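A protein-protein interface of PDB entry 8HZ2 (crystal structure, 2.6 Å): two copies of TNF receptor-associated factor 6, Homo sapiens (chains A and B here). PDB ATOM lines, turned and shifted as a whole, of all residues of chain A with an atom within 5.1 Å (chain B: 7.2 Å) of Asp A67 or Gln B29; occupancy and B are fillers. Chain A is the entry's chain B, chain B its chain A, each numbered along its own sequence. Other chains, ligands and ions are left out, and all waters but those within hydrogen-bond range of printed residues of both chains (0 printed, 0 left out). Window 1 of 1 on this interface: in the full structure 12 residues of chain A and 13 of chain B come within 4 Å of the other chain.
The backbone carbonyl oxygen of Pro B31 lies within hydrogen-bond range of the side-chain amide nitrogen of Asn A68 (3.2 Å).
OE1 of Gln B29 lies within hydrogen-bond range of N of Asn A68 (2.9 Å).
The side-chain amide nitrogen (NE2) of Gln B29 sits at hydrogen-bond distance from the side-chain carboxylate (OD1) of Asp A67.
OD1 of Asp B67 lies within hydrogen-bond range of NE2 of Gln A29, at 3.0 Å.
OE1 of Gln B29 sits at hydrogen-bond distance from N of Phe A69 (3.1 Å).
The guanidinium group (NH2) of Arg A35 lies close to the guanidinium group (NH2) of Arg B35, at 3.1 Å.
OD2 of Asp A67 is in salt-bridge range of NE of Arg A35.
The side-chain carboxylate (OD1) of Asp B67 lies close to the backbone NH (N) of Phe B69, at 3.5 Å.
OD2 of Asp A67 sits at hydrogen-bond distance from NE2 of Gln A29 (2.5 Å).
OD2 of Asp B67 sits at hydrogen-bond distance from NE2 of Gln B29 (3.1 Å).
The backbone NH of Gln A29 is in hydrogen-bond range of the backbone carbonyl oxygen of Phe A65, at 2.8 Å.
N of Ala A70 sits at hydrogen-bond distance from OD1 of Asp A67 (3.2 Å).
Gln A29 touches Phe B65 (CB to CZ, 3.5 Å).
Phe B69 touches Gln A29.
Arg A35 touches Phe B69 (NH1 to CE1, 3.3 Å).
Phe A65 touches Phe B65 (CD2 to CD1, 3.4 Å).
Gln B29 touches Pro A66 (OE1 to O, 3.7 Å).
Asn A68 touches Gly B33.
Gly B33 touches Phe A69.
Phe A69 touches Arg B35 (CE2 to NH1, 3.3 Å).
Printed residues of chain B within 4 Å of Arg A35: Arg B35 (3.1 Å) and Phe B69 (3.3 Å).
Of the printed residues of chain B, Phe A65 touches Phe B65.
Asp A67 touches one residue of chain B.
Printed residues of chain B within 4 Å of Asn A68: Gln B29, Pro B31 and Gly B33.
Gln B29 touches just these residues of chain A: Pro A66, Asp A67, Asn A68 and Phe A69.
Pro B66 touches none of the printed residues of chain A.
Of the printed residues of chain A, Phe B69 touches Gln A29 (3.7 Å) and Arg A35 (3.3 Å).
The nearest residue of chain A that does not touch Gln B29 is Gln A29 (4.3 Å).
Printed residues of chain B that touch a printed residue of chain A: Gln B29, Pro B31, Gly B33, Arg B35, Phe B65, Asp B67 and Phe B69.
Hydrophobic or aromatic side chains of chain B that line the printed part of chain A: Phe B65 and Phe B69.
Printed residues of chain A that touch a printed residue of chain B: Gln A29, Arg A35, Phe A65, Pro A66, Asp A67, Asn A68 and Phe A69.
Hydrophobic or aromatic side chains of chain A that line the printed part of chain B: Phe A65 and Phe A69.
Among the printed residues, 14 pairs touch across the chains.
Among the printed residues, no Asp or Glu carboxylate lies within 4 Å of a Lys or Arg side-chain nitrogen of the other chain.
Gln A29 touches Phe B65, but with the chains exchanged Phe A65 does not touch Gln B29 (6.8 Å).
Gln A29 touches Phe B69, and with the chains exchanged Phe A69 touches Gln B29.
Arg A35 touches Phe B69, and with the chains exchanged Phe A69 touches Arg B35.
Phe B65 touches its own counterpart, Phe A65.
Positions printed for both chains: 27, 28, 29, 35, 65, 66, 67, 69 and 70.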
ATOM      1  N   ALA A  27      -3.849  -8.133  -5.435  1.00  0.00           N
ATOM      2  CA  ALA A  27      -4.724  -9.074  -4.746  1.00  0.00           C
ATOM      3  C   ALA A  27      -5.616  -8.381  -3.722  1.00  0.00           C
ATOM      4  O   ALA A  27      -5.177  -7.501  -2.979  1.00  0.00           O
ATOM      5  CB  ALA A  27      -3.892 -10.158  -4.059  1.00  0.00           C
ATOM      6  N   VAL A  28      -6.883  -8.796  -3.692  1.00  0.00           N
ATOM      7  CA  VAL A  28      -7.843  -8.355  -2.690  1.00  0.00           C
ATOM      8  C   VAL A  28      -8.523  -9.587  -2.106  1.00  0.00           C
ATOM      9  O   VAL A  28      -8.583 -10.645  -2.740  1.00  0.00           O
ATOM     10  CB  VAL A  28      -8.891  -7.372  -3.264  1.00  0.00           C
ATOM     11  CG1 VAL A  28      -8.229  -6.066  -3.676  1.00  0.00           C
ATOM     12  CG2 VAL A  28      -9.628  -8.001  -4.436  1.00  0.00           C
ATOM     13  N   GLN A  29      -9.033  -9.446  -0.885  1.00  0.00           N
ATOM     14  CA  GLN A  29      -9.643 -10.552  -0.159  1.00  0.00           C
ATOM     15  C   GLN A  29     -11.078 -10.217   0.221  1.00  0.00           C
ATOM     16  O   GLN A  29     -11.378  -9.093   0.639  1.00  0.00           O
ATOM     17  CB  GLN A  29      -8.850 -10.895   1.106  1.00  0.00           C
ATOM     18  CG  GLN A  29      -8.099 -12.214   1.033  1.00  0.00           C
ATOM     19  CD  GLN A  29      -7.625 -12.699   2.392  1.00  0.00           C
ATOM     20  OE1 GLN A  29      -8.396 -12.743   3.351  1.00  0.00           O
ATOM     21  NE2 GLN A  29      -6.351 -13.066   2.478  1.00  0.00           N
ATOM     22  N   ARG A  35      -9.572 -14.927  -2.481  1.00  0.00           N
ATOM     23  CA  ARG A  35      -8.679 -13.962  -3.108  1.00  0.00           C
ATOM     24  C   ARG A  35      -9.022 -13.816  -4.584  1.00  0.00           C
ATOM     25  O   ARG A  35      -9.223 -14.816  -5.280  1.00  0.00           O
ATOM     26  CB  ARG A  35      -7.218 -14.396  -2.953  1.00  0.00           C
ATOM     27  CG  ARG A  35      -6.682 -14.307  -1.533  1.00  0.00           C
ATOM     28  CD  ARG A  35      -5.446 -15.174  -1.355  1.00  0.00           C
ATOM     29  NE  ARG A  35      -4.707 -14.826  -0.148  1.00  0.00           N
ATOM     30  CZ  ARG A  35      -3.718 -15.547   0.358  1.00  0.00           C
ATOM     31  NH1 ARG A  35      -3.339 -16.687  -0.197  1.00  0.00           N
ATOM     32  NH2 ARG A  35      -3.093 -15.115   1.450  1.00  0.00           N
ATOM     33  N   PHE A  65     -10.696  -5.782   0.838  1.00  0.00           N
ATOM     34  CA  PHE A  65      -9.466  -5.148   1.284  1.00  0.00           C
ATOM     35  C   PHE A  65      -8.288  -5.737   0.528  1.00  0.00           C
ATOM     36  O   PHE A  65      -8.348  -6.893   0.091  1.00  0.00           O
ATOM     37  CB  PHE A  65      -9.272  -5.317   2.796  1.00  0.00           C
ATOM     38  CG  PHE A  65     -10.130  -4.402   3.613  1.00  0.00           C
ATOM     39  CD1 PHE A  65      -9.775  -3.076   3.781  1.00  0.00           C
ATOM     40  CD2 PHE A  65     -11.292  -4.863   4.204  1.00  0.00           C
ATOM     41  CE1 PHE A  65     -10.560  -2.228   4.528  1.00  0.00           C
ATOM     42  CE2 PHE A  65     -12.082  -4.021   4.952  1.00  0.00           C
ATOM     43  CZ  PHE A  65     -11.716  -2.701   5.115  1.00  0.00           C
ATOM     44  N   PRO A  66      -7.202  -4.972   0.361  1.00  0.00           N
ATOM     45  CA  PRO A  66      -6.048  -5.477  -0.390  1.00  0.00           C
ATOM     46  C   PRO A  66      -5.247  -6.505   0.392  1.00  0.00           C
ATOM     47  O   PRO A  66      -4.642  -6.181   1.419  1.00  0.00           O
ATOM     48  CB  PRO A  66      -5.226  -4.210  -0.658  1.00  0.00           C
ATOM     49  CG  PRO A  66      -5.608  -3.273   0.440  1.00  0.00           C
ATOM     50  CD  PRO A  66      -7.053  -3.552   0.729  1.00  0.00           C
ATOM     51  N   ASP A  67      -5.231  -7.750  -0.091  1.00  0.00           N
ATOM     52  CA  ASP A  67      -4.417  -8.811   0.507  1.00  0.00           C
ATOM     53  C   ASP A  67      -2.968  -8.583   0.083  1.00  0.00           C
ATOM     54  O   ASP A  67      -2.437  -9.219  -0.831  1.00  0.00           O
ATOM     55  CB  ASP A  67      -4.922 -10.187   0.087  1.00  0.00           C
ATOM     56  CG  ASP A  67      -4.253 -11.326   0.852  1.00  0.00           C
ATOM     57  OD1 ASP A  67      -3.313 -11.064   1.631  1.00  0.00           O
ATOM     58  OD2 ASP A  67      -4.675 -12.490   0.673  1.00  0.00           O
ATOM     59  N   ASN A  68      -2.320  -7.638   0.765  1.00  0.00           N
ATOM     60  CA  ASN A  68      -0.944  -7.269   0.453  1.00  0.00           C
ATOM     61  C   ASN A  68       0.074  -8.316   0.895  1.00  0.00           C
ATOM     62  O   ASN A  68       1.256  -8.179   0.555  1.00  0.00           O
ATOM     63  CB  ASN A  68      -0.616  -5.910   1.077  1.00  0.00           C
ATOM     64  CG  ASN A  68      -1.015  -4.748   0.182  1.00  0.00           C
ATOM     65  OD1 ASN A  68      -0.837  -4.803  -1.034  1.00  0.00           O
ATOM     66  ND2 ASN A  68      -1.556  -3.694   0.779  1.00  0.00           N
ATOM     67  N   PHE A  69      -0.338  -9.344   1.644  1.00  0.00           N
ATOM     68  CA  PHE A  69       0.557 -10.468   1.889  1.00  0.00           C
ATOM     69  C   PHE A  69       0.600 -11.407   0.692  1.00  0.00           C
ATOM     70  O   PHE A  69       1.678 -11.861   0.294  1.00  0.00           O
ATOM     71  CB  PHE A  69       0.132 -11.238   3.141  1.00  0.00           C
ATOM     72  CG  PHE A  69       1.091 -12.333   3.525  1.00  0.00           C
ATOM     73  CD1 PHE A  69       2.205 -12.050   4.294  1.00  0.00           C
ATOM     74  CD2 PHE A  69       0.887 -13.638   3.106  1.00  0.00           C
ATOM     75  CE1 PHE A  69       3.097 -13.043   4.645  1.00  0.00           C
ATOM     76  CE2 PHE A  69       1.777 -14.640   3.454  1.00  0.00           C
ATOM     77  CZ  PHE A  69       2.882 -14.341   4.226  1.00  0.00           C
ATOM     78  N   ALA A  70      -0.565 -11.716   0.114  1.00  0.00           N
ATOM     79  CA  ALA A  70      -0.596 -12.537  -1.090  1.00  0.00           C
ATOM     80  C   ALA A  70       0.104 -11.835  -2.245  1.00  0.00           C
ATOM     81  O   ALA A  70       0.821 -12.471  -3.027  1.00  0.00           O
ATOM     82  CB  ALA A  70      -2.040 -12.877  -1.459  1.00  0.00           C
ATOM     83  N   LYS A  71      -0.089 -10.520  -2.362  1.00  0.00           N
ATOM     84  CA  LYS A  71       0.551  -9.756  -3.427  1.00  0.00           C
ATOM     85  C   LYS A  71       2.069  -9.804  -3.309  1.00  0.00           C
ATOM     86  O   LYS A  71       2.774  -9.937  -4.316  1.00  0.00           O
ATOM     87  CB  LYS A  71       0.049  -8.312  -3.391  1.00  0.00           C
ATOM     88  CG  LYS A  71       0.727  -7.356  -4.360  1.00  0.00           C
ATOM     89  CD  LYS A  71       0.254  -5.929  -4.110  1.00  0.00           C
ATOM     90  CE  LYS A  71       0.961  -4.930  -5.008  1.00  0.00           C
ATOM     91  NZ  LYS A  71       0.588  -3.528  -4.668  1.00  0.00           N
ATOM     92  N   GLU B  26      -7.200 -16.350  14.983  1.00  0.00           N
ATOM     93  CA  GLU B  26      -8.047 -15.307  14.407  1.00  0.00           C
ATOM     94  C   GLU B  26      -7.196 -14.315  13.615  1.00  0.00           C
ATOM     95  O   GLU B  26      -7.097 -13.130  13.940  1.00  0.00           O
ATOM     96  CB  GLU B  26      -8.865 -14.602  15.494  1.00  0.00           C
ATOM     97  CG  GLU B  26      -9.721 -15.541  16.325  1.00  0.00           C
ATOM     98  CD  GLU B  26     -10.723 -16.303  15.481  1.00  0.00           C
ATOM     99  OE1 GLU B  26     -11.410 -15.664  14.657  1.00  0.00           O
ATOM    100  OE2 GLU B  26     -10.815 -17.539  15.634  1.00  0.00           O
ATOM    101  N   ALA B  27      -6.567 -14.837  12.564  1.00  0.00           N
ATOM    102  CA  ALA B  27      -5.545 -14.088  11.843  1.00  0.00           C
ATOM    103  C   ALA B  27      -6.120 -12.832  11.199  1.00  0.00           C
ATOM    104  O   ALA B  27      -7.115 -12.889  10.471  1.00  0.00           O
ATOM    105  CB  ALA B  27      -4.903 -14.981  10.780  1.00  0.00           C
ATOM    106  N   VAL B  28      -5.488 -11.694  11.474  1.00  0.00           N
ATOM    107  CA  VAL B  28      -5.835 -10.429  10.846  1.00  0.00           C
ATOM    108  C   VAL B  28      -4.594  -9.886  10.152  1.00  0.00           C
ATOM    109  O   VAL B  28      -3.458 -10.212  10.505  1.00  0.00           O
ATOM    110  CB  VAL B  28      -6.393  -9.404  11.851  1.00  0.00           C
ATOM    111  CG1 VAL B  28      -7.619  -9.970  12.537  1.00  0.00           C
ATOM    112  CG2 VAL B  28      -5.326  -9.012  12.864  1.00  0.00           C
ATOM    113  N   GLN B  29      -4.826  -9.046   9.148  1.00  0.00           N
ATOM    114  CA  GLN B  29      -3.767  -8.524   8.299  1.00  0.00           C
ATOM    115  C   GLN B  29      -3.680  -7.010   8.441  1.00  0.00           C
ATOM    116  O   GLN B  29      -4.676  -6.333   8.707  1.00  0.00           O
ATOM    117  CB  GLN B  29      -4.003  -8.912   6.830  1.00  0.00           C
ATOM    118  CG  GLN B  29      -2.831  -8.641   5.903  1.00  0.00           C
ATOM    119  CD  GLN B  29      -3.044  -9.205   4.512  1.00  0.00           C
ATOM    120  OE1 GLN B  29      -2.713  -8.563   3.515  1.00  0.00           O
ATOM    121  NE2 GLN B  29      -3.595 -10.413   4.437  1.00  0.00           N
ATOM    122  N   THR B  30      -2.476  -6.492   8.272  1.00  0.00           N
ATOM    123  CA  THR B  30      -2.202  -5.068   8.336  1.00  0.00           C
ATOM    124  C   THR B  30      -2.259  -4.451   6.945  1.00  0.00           C
ATOM    125  O   THR B  30      -2.182  -5.158   5.933  1.00  0.00           O
ATOM    126  CB  THR B  30      -0.829  -4.837   8.960  1.00  0.00           C
ATOM    127  OG1 THR B  30       0.157  -5.576   8.226  1.00  0.00           O
ATOM    128  CG2 THR B  30      -0.822  -5.297  10.408  1.00  0.00           C
ATOM    129  N   PRO B  31      -2.411  -3.127   6.853  1.00  0.00           N
ATOM    130  CA  PRO B  31      -2.313  -2.479   5.538  1.00  0.00           C
ATOM    131  C   PRO B  31      -0.949  -2.641   4.889  1.00  0.00           C
ATOM    132  O   PRO B  31      -0.843  -2.497   3.666  1.00  0.00           O
ATOM    133  CB  PRO B  31      -2.619  -1.007   5.849  1.00  0.00           C
ATOM    134  CG  PRO B  31      -3.431  -1.055   7.097  1.00  0.00           C
ATOM    135  CD  PRO B  31      -2.843  -2.181   7.894  1.00  0.00           C
ATOM    136  N   CYS B  32       0.092  -2.957   5.662  1.00  0.00           N
ATOM    137  CA  CYS B  32       1.432  -3.139   5.124  1.00  0.00           C
ATOM    138  C   CYS B  32       1.720  -4.568   4.685  1.00  0.00           C
ATOM    139  O   CYS B  32       2.715  -4.790   3.987  1.00  0.00           O
ATOM    140  CB  CYS B  32       2.481  -2.699   6.152  1.00  0.00           C
ATOM    141  SG  CYS B  32       2.156  -3.251   7.838  1.00  0.00           S
ATOM    142  N   GLY B  33       0.897  -5.541   5.074  1.00  0.00           N
ATOM    143  CA  GLY B  33       1.027  -6.875   4.516  1.00  0.00           C
ATOM    144  C   GLY B  33       1.504  -7.961   5.458  1.00  0.00           C
ATOM    145  O   GLY B  33       1.906  -9.036   5.002  1.00  0.00           O
ATOM    146  N   HIS B  34       1.484  -7.708   6.764  1.00  0.00           N
ATOM    147  CA  HIS B  34       2.026  -8.638   7.746  1.00  0.00           C
ATOM    148  C   HIS B  34       0.912  -9.155   8.650  1.00  0.00           C
ATOM    149  O   HIS B  34       0.089  -8.374   9.140  1.00  0.00           O
ATOM    150  CB  HIS B  34       3.137  -7.964   8.557  1.00  0.00           C
ATOM    151  CG  HIS B  34       4.340  -7.603   7.740  1.00  0.00           C
ATOM    152  ND1 HIS B  34       4.903  -6.345   7.753  1.00  0.00           N
ATOM    153  CD2 HIS B  34       5.085  -8.340   6.880  1.00  0.00           C
ATOM    154  CE1 HIS B  34       5.945  -6.325   6.940  1.00  0.00           C
ATOM    155  NE2 HIS B  34       6.076  -7.522   6.397  1.00  0.00           N
ATOM    156  N   ARG B  35       0.887 -10.472   8.859  1.00  0.00           N
ATOM    157  CA  ARG B  35      -0.193 -11.135   9.581  1.00  0.00           C
ATOM    158  C   ARG B  35       0.117 -11.229  11.070  1.00  0.00           C
ATOM    159  O   ARG B  35       1.269 -11.419  11.469  1.00  0.00           O
ATOM    160  CB  ARG B  35      -0.426 -12.541   9.024  1.00  0.00           C
ATOM    161  CG  ARG B  35      -0.720 -12.606   7.536  1.00  0.00           C
ATOM    162  CD  ARG B  35      -0.269 -13.944   6.973  1.00  0.00           C
ATOM    163  NE  ARG B  35      -1.088 -14.371   5.847  1.00  0.00           N
ATOM    164  CZ  ARG B  35      -0.948 -15.530   5.219  1.00  0.00           C
ATOM    165  NH1 ARG B  35      -0.010 -16.395   5.568  1.00  0.00           N
ATOM    166  NH2 ARG B  35      -1.769 -15.828   4.217  1.00  0.00           N
ATOM    167  N   PHE B  36      -0.924 -11.102  11.892  1.00  0.00           N
ATOM    168  CA  PHE B  36      -0.795 -11.226  13.336  1.00  0.00           C
ATOM    169  C   PHE B  36      -2.047 -11.879  13.898  1.00  0.00           C
ATOM    170  O   PHE B  36      -3.115 -11.854  13.280  1.00  0.00           O
ATOM    171  CB  PHE B  36      -0.586  -9.867  14.020  1.00  0.00           C
ATOM    172  CG  PHE B  36       0.561  -9.077  13.468  1.00  0.00           C
ATOM    173  CD1 PHE B  36       1.822  -9.180  14.028  1.00  0.00           C
ATOM    174  CD2 PHE B  36       0.377  -8.223  12.393  1.00  0.00           C
ATOM    175  CE1 PHE B  36       2.878  -8.450  13.523  1.00  0.00           C
ATOM    176  CE2 PHE B  36       1.432  -7.496  11.883  1.00  0.00           C
ATOM    177  CZ  PHE B  36       2.682  -7.610  12.447  1.00  0.00           C
ATOM    178  N   ILE B  41      -1.861  -8.386  17.994  1.00  0.00           N
ATOM    179  CA  ILE B  41      -1.656  -7.053  17.438  1.00  0.00           C
ATOM    180  C   ILE B  41      -2.487  -6.019  18.191  1.00  0.00           C
ATOM    181  O   ILE B  41      -2.053  -4.875  18.367  1.00  0.00           O
ATOM    182  CB  ILE B  41      -1.946  -7.056  15.925  1.00  0.00           C
ATOM    183  CG1 ILE B  41      -1.530  -5.725  15.296  1.00  0.00           C
ATOM    184  CG2 ILE B  41      -3.404  -7.389  15.646  1.00  0.00           C
ATOM    185  CD1 ILE B  41      -0.046  -5.436  15.417  1.00  0.00           C
ATOM    186  N   LEU B  59      -0.352   2.111  11.659  1.00  0.00           N
ATOM    187  CA  LEU B  59      -1.349   1.056  11.787  1.00  0.00           C
ATOM    188  C   LEU B  59      -2.363   1.424  12.857  1.00  0.00           C
ATOM    189  O   LEU B  59      -1.987   1.749  13.986  1.00  0.00           O
ATOM    190  CB  LEU B  59      -0.683  -0.283  12.131  1.00  0.00           C
ATOM    191  CG  LEU B  59      -1.616  -1.420  12.554  1.00  0.00           C
ATOM    192  CD1 LEU B  59      -2.603  -1.761  11.448  1.00  0.00           C
ATOM    193  CD2 LEU B  59      -0.811  -2.645  12.956  1.00  0.00           C
ATOM    194  N   LEU B  60      -3.642   1.372  12.497  1.00  0.00           N
ATOM    195  CA  LEU B  60      -4.741   1.550  13.432  1.00  0.00           C
ATOM    196  C   LEU B  60      -5.562   0.270  13.526  1.00  0.00           C
ATOM    197  O   LEU B  60      -5.470  -0.619  12.674  1.00  0.00           O
ATOM    198  CB  LEU B  60      -5.638   2.723  13.019  1.00  0.00           C
ATOM    199  CG  LEU B  60      -5.017   4.120  13.096  1.00  0.00           C
ATOM    200  CD1 LEU B  60      -6.020   5.168  12.649  1.00  0.00           C
ATOM    201  CD2 LEU B  60      -4.519   4.419  14.502  1.00  0.00           C
ATOM    202  N   GLN B  63      -8.138  -0.089  10.958  1.00  0.00           N
ATOM    203  CA  GLN B  63      -7.448  -0.423   9.720  1.00  0.00           C
ATOM    204  C   GLN B  63      -7.052  -1.891   9.642  1.00  0.00           C
ATOM    205  O   GLN B  63      -6.496  -2.313   8.622  1.00  0.00           O
ATOM    206  CB  GLN B  63      -6.205   0.455   9.560  1.00  0.00           C
ATOM    207  CG  GLN B  63      -6.501   1.945   9.530  1.00  0.00           C
ATOM    208  CD  GLN B  63      -5.242   2.782   9.441  1.00  0.00           C
ATOM    209  OE1 GLN B  63      -4.140   2.292   9.685  1.00  0.00           O
ATOM    210  NE2 GLN B  63      -5.399   4.052   9.088  1.00  0.00           N
ATOM    211  N   LEU B  64      -7.315  -2.673  10.685  1.00  0.00           N
ATOM    212  CA  LEU B  64      -7.084  -4.105  10.616  1.00  0.00           C
ATOM    213  C   LEU B  64      -8.156  -4.773   9.764  1.00  0.00           C
ATOM    214  O   LEU B  64      -9.212  -4.202   9.478  1.00  0.00           O
ATOM    215  CB  LEU B  64      -7.066  -4.724  12.013  1.00  0.00           C
ATOM    216  CG  LEU B  64      -5.770  -4.562  12.806  1.00  0.00           C
ATOM    217  CD1 LEU B  64      -5.915  -5.210  14.169  1.00  0.00           C
ATOM    218  CD2 LEU B  64      -4.604  -5.166  12.042  1.00  0.00           C
ATOM    219  N   PHE B  65      -7.871  -6.005   9.368  1.00  0.00           N
ATOM    220  CA  PHE B  65      -8.743  -6.744   8.469  1.00  0.00           C
ATOM    221  C   PHE B  65      -8.527  -8.239   8.665  1.00  0.00           C
ATOM    222  O   PHE B  65      -7.392  -8.720   8.559  1.00  0.00           O
ATOM    223  CB  PHE B  65      -8.476  -6.326   7.023  1.00  0.00           C
ATOM    224  CG  PHE B  65      -8.812  -7.377   6.012  1.00  0.00           C
ATOM    225  CD1 PHE B  65     -10.130  -7.658   5.699  1.00  0.00           C
ATOM    226  CD2 PHE B  65      -7.807  -8.074   5.363  1.00  0.00           C
ATOM    227  CE1 PHE B  65     -10.441  -8.623   4.765  1.00  0.00           C
ATOM    228  CE2 PHE B  65      -8.113  -9.042   4.427  1.00  0.00           C
ATOM    229  CZ  PHE B  65      -9.432  -9.315   4.127  1.00  0.00           C
ATOM    230  N   PRO B  66      -9.579  -8.998   8.970  1.00  0.00           N
ATOM    231  CA  PRO B  66      -9.408 -10.439   9.197  1.00  0.00           C
ATOM    232  C   PRO B  66      -8.863 -11.136   7.957  1.00  0.00           C
ATOM    233  O   PRO B  66      -9.227 -10.807   6.826  1.00  0.00           O
ATOM    234  CB  PRO B  66     -10.825 -10.914   9.539  1.00  0.00           C
ATOM    235  CG  PRO B  66     -11.732  -9.877   8.950  1.00  0.00           C
ATOM    236  CD  PRO B  66     -10.988  -8.581   9.054  1.00  0.00           C
ATOM    237  N   ASP B  67      -7.972 -12.099   8.180  1.00  0.00           N
ATOM    238  CA  ASP B  67      -7.417 -12.928   7.112  1.00  0.00           C
ATOM    239  C   ASP B  67      -8.023 -14.319   7.274  1.00  0.00           C
ATOM    240  O   ASP B  67      -7.440 -15.211   7.894  1.00  0.00           O
ATOM    241  CB  ASP B  67      -5.867 -12.962   7.162  1.00  0.00           C
ATOM    242  CG  ASP B  67      -5.248 -13.551   5.900  1.00  0.00           C
ATOM    243  OD1 ASP B  67      -5.941 -14.296   5.179  1.00  0.00           O
ATOM    244  OD2 ASP B  67      -4.060 -13.270   5.632  1.00  0.00           O
ATOM    245  N   PHE B  69      -8.678 -16.366   4.762  1.00  0.00           N
ATOM    246  CA  PHE B  69      -7.969 -17.302   3.899  1.00  0.00           C
ATOM    247  C   PHE B  69      -6.824 -17.968   4.653  1.00  0.00           C
ATOM    248  O   PHE B  69      -6.616 -19.181   4.537  1.00  0.00           O
ATOM    249  CB  PHE B  69      -7.452 -16.581   2.657  1.00  0.00           C
ATOM    250  CG  PHE B  69      -7.090 -17.502   1.528  1.00  0.00           C
ATOM    251  CD1 PHE B  69      -5.874 -18.167   1.518  1.00  0.00           C
ATOM    252  CD2 PHE B  69      -7.965 -17.699   0.474  1.00  0.00           C
ATOM    253  CE1 PHE B  69      -5.541 -19.016   0.480  1.00  0.00           C
ATOM    254  CE2 PHE B  69      -7.638 -18.545  -0.569  1.00  0.00           C
ATOM    255  CZ  PHE B  69      -6.424 -19.204  -0.567  1.00  0.00           C
ATOM    256  N   ALA B  70      -6.066 -17.187   5.426  1.00  0.00           N
ATOM    257  CA  ALA B  70      -5.075 -17.773   6.321  1.00  0.00           C
ATOM    258  C   ALA B  70      -5.745 -18.558   7.441  1.00  0.00           C
ATOM    259  O   ALA B  70      -5.256 -19.619   7.843  1.00  0.00           O
ATOM    260  CB  ALA B  70      -4.169 -16.684   6.895  1.00  0.00           C
